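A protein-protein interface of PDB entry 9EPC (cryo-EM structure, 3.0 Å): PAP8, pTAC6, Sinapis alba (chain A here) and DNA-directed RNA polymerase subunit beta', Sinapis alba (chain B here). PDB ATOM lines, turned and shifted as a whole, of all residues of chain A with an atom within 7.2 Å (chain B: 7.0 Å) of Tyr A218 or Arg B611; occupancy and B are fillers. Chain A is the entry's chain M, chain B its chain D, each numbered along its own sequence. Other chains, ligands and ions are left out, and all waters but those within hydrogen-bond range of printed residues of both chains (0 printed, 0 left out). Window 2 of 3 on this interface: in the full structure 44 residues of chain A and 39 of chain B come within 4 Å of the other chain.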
ATOM      1  N   TYR A 203      28.262  -0.730 -29.381  1.00  0.00           N
ATOM      2  CA  TYR A 203      27.570  -1.913 -29.874  1.00  0.00           C
ATOM      3  C   TYR A 203      26.636  -1.497 -31.001  1.00  0.00           C
ATOM      4  O   TYR A 203      25.771  -0.637 -30.808  1.00  0.00           O
ATOM      5  CB  TYR A 203      26.783  -2.596 -28.760  1.00  0.00           C
ATOM      6  CG  TYR A 203      27.627  -3.411 -27.813  1.00  0.00           C
ATOM      7  CD1 TYR A 203      28.228  -2.826 -26.712  1.00  0.00           C
ATOM      8  CD2 TYR A 203      27.816  -4.768 -28.018  1.00  0.00           C
ATOM      9  CE1 TYR A 203      28.997  -3.566 -25.846  1.00  0.00           C
ATOM     10  CE2 TYR A 203      28.581  -5.518 -27.154  1.00  0.00           C
ATOM     11  CZ  TYR A 203      29.169  -4.911 -26.069  1.00  0.00           C
ATOM     12  OH  TYR A 203      29.938  -5.654 -25.202  1.00  0.00           O
ATOM     13  N   VAL A 205      23.907  -2.803 -32.564  1.00  0.00           N
ATOM     14  CA  VAL A 205      22.778  -3.727 -32.596  1.00  0.00           C
ATOM     15  C   VAL A 205      21.834  -3.267 -33.699  1.00  0.00           C
ATOM     16  O   VAL A 205      21.194  -2.219 -33.586  1.00  0.00           O
ATOM     17  CB  VAL A 205      22.063  -3.795 -31.243  1.00  0.00           C
ATOM     18  CG1 VAL A 205      20.851  -4.702 -31.337  1.00  0.00           C
ATOM     19  CG2 VAL A 205      23.014  -4.289 -30.171  1.00  0.00           C
ATOM     20  N   THR A 206      21.748  -4.048 -34.768  1.00  0.00           N
ATOM     21  CA  THR A 206      20.940  -3.709 -35.927  1.00  0.00           C
ATOM     22  C   THR A 206      19.966  -4.837 -36.230  1.00  0.00           C
ATOM     23  O   THR A 206      20.138  -5.973 -35.783  1.00  0.00           O
ATOM     24  CB  THR A 206      21.814  -3.436 -37.155  1.00  0.00           C
ATOM     25  OG1 THR A 206      20.979  -3.254 -38.304  1.00  0.00           O
ATOM     26  CG2 THR A 206      22.759  -4.599 -37.400  1.00  0.00           C
ATOM     27  N   GLU A 207      18.931  -4.506 -37.001  1.00  0.00           N
ATOM     28  CA  GLU A 207      17.921  -5.469 -37.429  1.00  0.00           C
ATOM     29  C   GLU A 207      18.094  -5.729 -38.918  1.00  0.00           C
ATOM     30  O   GLU A 207      17.565  -4.980 -39.752  1.00  0.00           O
ATOM     31  CB  GLU A 207      16.513  -4.953 -37.123  1.00  0.00           C
ATOM     32  CG  GLU A 207      16.218  -4.826 -35.641  1.00  0.00           C
ATOM     33  CD  GLU A 207      14.830  -4.286 -35.369  1.00  0.00           C
ATOM     34  OE1 GLU A 207      14.231  -3.694 -36.291  1.00  0.00           O
ATOM     35  OE2 GLU A 207      14.336  -4.456 -34.236  1.00  0.00           O
ATOM     36  N   PRO A 208      18.820  -6.772 -39.304  1.00  0.00           N
ATOM     37  CA  PRO A 208      19.065  -7.029 -40.723  1.00  0.00           C
ATOM     38  C   PRO A 208      17.786  -7.435 -41.429  1.00  0.00           C
ATOM     39  O   PRO A 208      16.845  -7.930 -40.790  1.00  0.00           O
ATOM     40  CB  PRO A 208      20.079  -8.183 -40.706  1.00  0.00           C
ATOM     41  CG  PRO A 208      20.622  -8.214 -39.320  1.00  0.00           C
ATOM     42  CD  PRO A 208      19.515  -7.740 -38.444  1.00  0.00           C
ATOM     43  N   ILE A 210      15.286  -9.784 -43.423  1.00  0.00           N
ATOM     44  CA  ILE A 210      15.054 -11.218 -43.312  1.00  0.00           C
ATOM     45  C   ILE A 210      14.596 -11.722 -44.671  1.00  0.00           C
ATOM     46  O   ILE A 210      13.486 -11.409 -45.120  1.00  0.00           O
ATOM     47  CB  ILE A 210      14.022 -11.544 -42.227  1.00  0.00           C
ATOM     48  CG1 ILE A 210      14.474 -10.986 -40.880  1.00  0.00           C
ATOM     49  CG2 ILE A 210      13.809 -13.043 -42.136  1.00  0.00           C
ATOM     50  CD1 ILE A 210      13.496 -11.238 -39.764  1.00  0.00           C
ATOM     51  N   ASP A 215      16.280 -16.479 -40.336  1.00  0.00           N
ATOM     52  CA  ASP A 215      17.308 -15.458 -40.260  1.00  0.00           C
ATOM     53  C   ASP A 215      17.221 -14.732 -38.920  1.00  0.00           C
ATOM     54  O   ASP A 215      16.129 -14.539 -38.382  1.00  0.00           O
ATOM     55  CB  ASP A 215      17.163 -14.460 -41.402  1.00  0.00           C
ATOM     56  CG  ASP A 215      18.122 -14.735 -42.538  1.00  0.00           C
ATOM     57  OD1 ASP A 215      19.211 -15.287 -42.277  1.00  0.00           O
ATOM     58  OD2 ASP A 215      17.791 -14.397 -43.692  1.00  0.00           O
ATOM     59  N   PRO A 216      18.359 -14.326 -38.357  1.00  0.00           N
ATOM     60  CA  PRO A 216      18.333 -13.671 -37.046  1.00  0.00           C
ATOM     61  C   PRO A 216      17.525 -12.384 -37.081  1.00  0.00           C
ATOM     62  O   PRO A 216      17.591 -11.611 -38.039  1.00  0.00           O
ATOM     63  CB  PRO A 216      19.814 -13.403 -36.757  1.00  0.00           C
ATOM     64  CG  PRO A 216      20.460 -13.380 -38.097  1.00  0.00           C
ATOM     65  CD  PRO A 216      19.718 -14.386 -38.918  1.00  0.00           C
ATOM     66  N   LEU A 217      16.752 -12.162 -36.018  1.00  0.00           N
ATOM     67  CA  LEU A 217      15.980 -10.930 -35.913  1.00  0.00           C
ATOM     68  C   LEU A 217      16.880  -9.728 -35.670  1.00  0.00           C
ATOM     69  O   LEU A 217      16.572  -8.622 -36.126  1.00  0.00           O
ATOM     70  CB  LEU A 217      14.946 -11.053 -34.797  1.00  0.00           C
ATOM     71  CG  LEU A 217      13.811 -12.045 -35.039  1.00  0.00           C
ATOM     72  CD1 LEU A 217      13.033 -12.282 -33.762  1.00  0.00           C
ATOM     73  CD2 LEU A 217      12.893 -11.531 -36.130  1.00  0.00           C
ATOM     74  N   TYR A 218      17.988  -9.923 -34.962  1.00  0.00           N
ATOM     75  CA  TYR A 218      18.923  -8.855 -34.656  1.00  0.00           C
ATOM     76  C   TYR A 218      20.341  -9.340 -34.909  1.00  0.00           C
ATOM     77  O   TYR A 218      20.624 -10.540 -34.892  1.00  0.00           O
ATOM     78  CB  TYR A 218      18.789  -8.388 -33.202  1.00  0.00           C
ATOM     79  CG  TYR A 218      19.375  -9.356 -32.203  1.00  0.00           C
ATOM     80  CD1 TYR A 218      18.703 -10.518 -31.858  1.00  0.00           C
ATOM     81  CD2 TYR A 218      20.601  -9.108 -31.604  1.00  0.00           C
ATOM     82  CE1 TYR A 218      19.235 -11.405 -30.947  1.00  0.00           C
ATOM     83  CE2 TYR A 218      21.140  -9.990 -30.692  1.00  0.00           C
ATOM     84  CZ  TYR A 218      20.454 -11.136 -30.368  1.00  0.00           C
ATOM     85  OH  TYR A 218      20.987 -12.018 -29.458  1.00  0.00           O
ATOM     86  N   LYS A 219      21.236  -8.386 -35.145  1.00  0.00           N
ATOM     87  CA  LYS A 219      22.659  -8.663 -35.304  1.00  0.00           C
ATOM     88  C   LYS A 219      23.422  -7.735 -34.372  1.00  0.00           C
ATOM     89  O   LYS A 219      23.529  -6.534 -34.639  1.00  0.00           O
ATOM     90  CB  LYS A 219      23.107  -8.470 -36.750  1.00  0.00           C
ATOM     91  CG  LYS A 219      24.597  -8.659 -36.963  1.00  0.00           C
ATOM     92  CD  LYS A 219      24.994  -8.301 -38.381  1.00  0.00           C
ATOM     93  CE  LYS A 219      26.500  -8.362 -38.562  1.00  0.00           C
ATOM     94  NZ  LYS A 219      26.910  -7.907 -39.920  1.00  0.00           N
ATOM     95  N   SER A 220      23.947  -8.287 -33.285  1.00  0.00           N
ATOM     96  CA  SER A 220      24.687  -7.518 -32.295  1.00  0.00           C
ATOM     97  C   SER A 220      26.178  -7.720 -32.519  1.00  0.00           C
ATOM     98  O   SER A 220      26.676  -8.847 -32.431  1.00  0.00           O
ATOM     99  CB  SER A 220      24.299  -7.933 -30.878  1.00  0.00           C
ATOM    100  OG  SER A 220      25.059  -7.221 -29.918  1.00  0.00           O
ATOM    101  N   GLU A 221      26.882  -6.631 -32.805  1.00  0.00           N
ATOM    102  CA  GLU A 221      28.324  -6.661 -32.987  1.00  0.00           C
ATOM    103  C   GLU A 221      28.927  -5.444 -32.304  1.00  0.00           C
ATOM    104  O   GLU A 221      28.298  -4.387 -32.218  1.00  0.00           O
ATOM    105  CB  GLU A 221      28.705  -6.681 -34.470  1.00  0.00           C
ATOM    106  CG  GLU A 221      28.144  -5.518 -35.261  1.00  0.00           C
ATOM    107  CD  GLU A 221      28.407  -5.646 -36.746  1.00  0.00           C
ATOM    108  OE1 GLU A 221      29.107  -6.602 -37.144  1.00  0.00           O
ATOM    109  OE2 GLU A 221      27.915  -4.795 -37.515  1.00  0.00           O
ATOM    110  N   TRP B 606      21.155  -7.913 -16.863  1.00  0.00           N
ATOM    111  CA  TRP B 606      20.966  -8.602 -18.130  1.00  0.00           C
ATOM    112  C   TRP B 606      21.882  -9.817 -18.192  1.00  0.00           C
ATOM    113  O   TRP B 606      23.108  -9.682 -18.132  1.00  0.00           O
ATOM    114  CB  TRP B 606      21.245  -7.656 -19.294  1.00  0.00           C
ATOM    115  CG  TRP B 606      20.807  -8.181 -20.612  1.00  0.00           C
ATOM    116  CD1 TRP B 606      21.603  -8.638 -21.615  1.00  0.00           C
ATOM    117  CD2 TRP B 606      19.461  -8.304 -21.077  1.00  0.00           C
ATOM    118  NE1 TRP B 606      20.838  -9.037 -22.680  1.00  0.00           N
ATOM    119  CE2 TRP B 606      19.518  -8.843 -22.374  1.00  0.00           C
ATOM    120  CE3 TRP B 606      18.215  -8.010 -20.524  1.00  0.00           C
ATOM    121  CZ2 TRP B 606      18.376  -9.096 -23.125  1.00  0.00           C
ATOM    122  CZ3 TRP B 606      17.083  -8.261 -21.270  1.00  0.00           C
ATOM    123  CH2 TRP B 606      17.170  -8.799 -22.557  1.00  0.00           C
ATOM    124  N   LEU B 608      21.571 -12.197 -20.787  1.00  0.00           N
ATOM    125  CA  LEU B 608      21.770 -12.567 -22.180  1.00  0.00           C
ATOM    126  C   LEU B 608      22.900 -11.730 -22.774  1.00  0.00           C
ATOM    127  O   LEU B 608      23.647 -11.052 -22.063  1.00  0.00           O
ATOM    128  CB  LEU B 608      20.470 -12.400 -22.960  1.00  0.00           C
ATOM    129  CG  LEU B 608      19.254 -13.127 -22.390  1.00  0.00           C
ATOM    130  CD1 LEU B 608      18.011 -12.792 -23.193  1.00  0.00           C
ATOM    131  CD2 LEU B 608      19.495 -14.624 -22.370  1.00  0.00           C
ATOM    132  N   ASP B 609      23.044 -11.780 -24.092  1.00  0.00           N
ATOM    133  CA  ASP B 609      24.017 -10.946 -24.774  1.00  0.00           C
ATOM    134  C   ASP B 609      23.468  -9.533 -24.951  1.00  0.00           C
ATOM    135  O   ASP B 609      22.324  -9.231 -24.603  1.00  0.00           O
ATOM    136  CB  ASP B 609      24.377 -11.545 -26.130  1.00  0.00           C
ATOM    137  CG  ASP B 609      23.188 -11.626 -27.060  1.00  0.00           C
ATOM    138  OD1 ASP B 609      22.056 -11.807 -26.564  1.00  0.00           O
ATOM    139  OD2 ASP B 609      23.381 -11.505 -28.287  1.00  0.00           O
ATOM    140  N   GLN B 610      24.303  -8.658 -25.502  1.00  0.00           N
ATOM    141  CA  GLN B 610      23.857  -7.308 -25.812  1.00  0.00           C
ATOM    142  C   GLN B 610      22.764  -7.358 -26.867  1.00  0.00           C
ATOM    143  O   GLN B 610      22.993  -7.806 -27.993  1.00  0.00           O
ATOM    144  CB  GLN B 610      25.030  -6.460 -26.295  1.00  0.00           C
ATOM    145  CG  GLN B 610      24.613  -5.117 -26.859  1.00  0.00           C
ATOM    146  CD  GLN B 610      23.905  -4.250 -25.844  1.00  0.00           C
ATOM    147  OE1 GLN B 610      23.007  -3.486 -26.188  1.00  0.00           O
ATOM    148  NE2 GLN B 610      24.312  -4.357 -24.585  1.00  0.00           N
ATOM    149  N   ARG B 611      21.572  -6.896 -26.500  1.00  0.00           N
ATOM    150  CA  ARG B 611      20.392  -7.083 -27.331  1.00  0.00           C
ATOM    151  C   ARG B 611      19.557  -5.827 -27.525  1.00  0.00           C
ATOM    152  O   ARG B 611      18.798  -5.766 -28.500  1.00  0.00           O
ATOM    153  CB  ARG B 611      19.507  -8.187 -26.730  1.00  0.00           C
ATOM    154  CG  ARG B 611      18.411  -8.700 -27.634  1.00  0.00           C
ATOM    155  CD  ARG B 611      17.817  -9.977 -27.074  1.00  0.00           C
ATOM    156  NE  ARG B 611      18.793 -11.057 -27.058  1.00  0.00           N
ATOM    157  CZ  ARG B 611      18.502 -12.325 -26.805  1.00  0.00           C
ATOM    158  NH1 ARG B 611      17.264 -12.712 -26.547  1.00  0.00           N
ATOM    159  NH2 ARG B 611      19.476 -13.230 -26.818  1.00  0.00           N
ATOM    160  N   VAL B 612      19.671  -4.824 -26.655  1.00  0.00           N
ATOM    161  CA  VAL B 612      18.838  -3.636 -26.772  1.00  0.00           C
ATOM    162  C   VAL B 612      19.273  -2.817 -27.980  1.00  0.00           C
ATOM    163  O   VAL B 612      20.458  -2.781 -28.340  1.00  0.00           O
ATOM    164  CB  VAL B 612      18.894  -2.806 -25.478  1.00  0.00           C
ATOM    165  CG1 VAL B 612      18.583  -3.681 -24.282  1.00  0.00           C
ATOM    166  CG2 VAL B 612      20.251  -2.154 -25.312  1.00  0.00           C
ATOM    167  N   ILE B 613      18.308  -2.166 -28.623  1.00  0.00           N
ATOM    168  CA  ILE B 613      18.572  -1.340 -29.795  1.00  0.00           C
ATOM    169  C   ILE B 613      18.726   0.099 -29.313  1.00  0.00           C
ATOM    170  O   ILE B 613      17.749   0.769 -28.978  1.00  0.00           O
ATOM    171  CB  ILE B 613      17.471  -1.470 -30.846  1.00  0.00           C
ATOM    172  CG1 ILE B 613      16.120  -1.726 -30.177  1.00  0.00           C
ATOM    173  CG2 ILE B 613      17.808  -2.570 -31.834  1.00  0.00           C
ATOM    174  CD1 ILE B 613      14.992  -1.926 -31.156  1.00  0.00           C
ATOM    175  N   ALA B 614      19.967   0.573 -29.279  1.00  0.00           N
ATOM    176  CA  ALA B 614      20.277   1.947 -28.932  1.00  0.00           C
ATOM    177  C   ALA B 614      21.196   2.522 -29.997  1.00  0.00           C
ATOM    178  O   ALA B 614      21.874   1.788 -30.720  1.00  0.00           O
ATOM    179  CB  ALA B 614      20.931   2.051 -27.550  1.00  0.00           C
ATOM    180  N   ILE B 650      26.265  -6.950 -17.504  1.00  0.00           N
ATOM    181  CA  ILE B 650      25.474  -5.975 -18.242  1.00  0.00           C
ATOM    182  C   ILE B 650      24.235  -5.630 -17.430  1.00  0.00           C
ATOM    183  O   ILE B 650      23.508  -6.524 -16.987  1.00  0.00           O
ATOM    184  CB  ILE B 650      25.072  -6.497 -19.632  1.00  0.00           C
ATOM    185  CG1 ILE B 650      26.314  -6.780 -20.474  1.00  0.00           C
ATOM    186  CG2 ILE B 650      24.172  -5.500 -20.333  1.00  0.00           C
ATOM    187  CD1 ILE B 650      26.001  -7.247 -21.873  1.00  0.00           C
ATOM    188  N   ILE B 652      20.834  -3.170 -17.825  1.00  0.00           N
ATOM    189  CA  ILE B 652      20.051  -2.364 -18.752  1.00  0.00           C
ATOM    190  C   ILE B 652      19.234  -1.359 -17.957  1.00  0.00           C
ATOM    191  O   ILE B 652      18.545  -1.725 -16.998  1.00  0.00           O
ATOM    192  CB  ILE B 652      19.136  -3.249 -19.614  1.00  0.00           C
ATOM    193  CG1 ILE B 652      19.944  -4.343 -20.305  1.00  0.00           C
ATOM    194  CG2 ILE B 652      18.400  -2.409 -20.638  1.00  0.00           C
ATOM    195  CD1 ILE B 652      20.955  -3.820 -21.285  1.00  0.00           C
ATOM    196  N   TYR B 662       8.550  -6.704 -23.791  1.00  0.00           N
ATOM    197  CA  TYR B 662       9.486  -7.740 -24.210  1.00  0.00           C
ATOM    198  C   TYR B 662       9.082  -9.100 -23.662  1.00  0.00           C
ATOM    199  O   TYR B 662       9.144 -10.108 -24.374  1.00  0.00           O
ATOM    200  CB  TYR B 662      10.901  -7.386 -23.762  1.00  0.00           C
ATOM    201  CG  TYR B 662      11.923  -8.440 -24.109  1.00  0.00           C
ATOM    202  CD1 TYR B 662      12.503  -8.480 -25.367  1.00  0.00           C
ATOM    203  CD2 TYR B 662      12.310  -9.393 -23.179  1.00  0.00           C
ATOM    204  CE1 TYR B 662      13.436  -9.440 -25.689  1.00  0.00           C
ATOM    205  CE2 TYR B 662      13.243 -10.357 -23.494  1.00  0.00           C
ATOM    206  CZ  TYR B 662      13.802 -10.375 -24.751  1.00  0.00           C
ATOM    207  OH  TYR B 662      14.735 -11.333 -25.071  1.00  0.00           O
ATOM    208  N   GLU B 666       8.153 -12.684 -25.666  1.00  0.00           N
ATOM    209  CA  GLU B 666       8.921 -13.885 -25.359  1.00  0.00           C
ATOM    210  C   GLU B 666       8.030 -14.982 -24.791  1.00  0.00           C
ATOM    211  O   GLU B 666       8.170 -16.154 -25.157  1.00  0.00           O
ATOM    212  CB  GLU B 666      10.049 -13.551 -24.386  1.00  0.00           C
ATOM    213  CG  GLU B 666      11.001 -14.701 -24.128  1.00  0.00           C
ATOM    214  CD  GLU B 666      12.050 -14.366 -23.087  1.00  0.00           C
ATOM    215  OE1 GLU B 666      11.802 -13.462 -22.262  1.00  0.00           O
ATOM    216  OE2 GLU B 666      13.123 -15.004 -23.094  1.00  0.00           O
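Of chain B, only Asp B609 (2.7 Å), Gln B610 (3.9 Å) and Arg B611 (3.3 Å) come within 4 Å of Tyr A218.
Printed residues of chain B within 4 Å of Tyr A203: Gln B610.
Printed residues of chain A within 4 Å of Val B612: Val A205 (3.5 Å).
Of the printed residues of chain A, Asp B609 touches Tyr A218 (2.7 Å).
Of the printed residues of chain B, Val A205 touches Gln B610 (3.8 Å), Arg B611 (3.7 Å), Val B612 (3.5 Å) and Ile B613 (3.7 Å).
Of the printed residues of chain B, Ser A220 touches Gln B610 (2.9 Å).
Asp A215 touches none of the printed residues of chain B.
The nearest residue of chain A that does not touch Arg B611 is Ser A220 (4.9 Å).
The nearest printed residue of chain B that does not touch Ser A220 is Asp B609 (4.5 Å).
Of the 12 printed residues of chain B, 5 touch a printed residue of chain A.
Printed residues of chain A that touch a printed residue of chain B: Tyr A203, Val A205, Tyr A218 and Ser A220.
Among the printed residues, no Asp or Glu carboxylate lies within 4 Å of a Lys or Arg side-chain nitrogen of the other chain.
The side-chain hydroxyl (OH) of Tyr A218 is in hydrogen-bond range of the guanidinium group (NH2) of Arg B611 (3.3 Å).
OG of Ser A220 sits at hydrogen-bond distance from O of Gln B610 (2.9 Å).
The side-chain carboxylate (OD2) of Asp B609 lies within hydrogen-bond range of the side-chain hydroxyl (OH) of Tyr A218 (2.7 Å).
NE1 of Trp B606 lies within hydrogen-bond range of O of Asp B609 (2.4 Å).
O of Val B612 lies close to OE1 of Gln B610 (3.4 Å).
NH1 of Arg B611 is in hydrogen-bond range of OH of Tyr B662, 3.2 Å away.
The side-chain carboxylate (OD1) of Asp B609 lies within salt-bridge range of the guanidinium group (NH2) of Arg B611, 3.0 Å away.
Among the printed residues, merely in contact across the chains: Tyr A203 with Gln B610 (3.4 Å), Val A205 with Val B612 (3.5 Å), Val A205 with Arg B611 (3.7 Å), Val A205 with Ile B613 (3.7 Å), Val A205 with Gln B610 (3.8 Å) and Tyr A218 with Gln B610 (3.9 Å).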
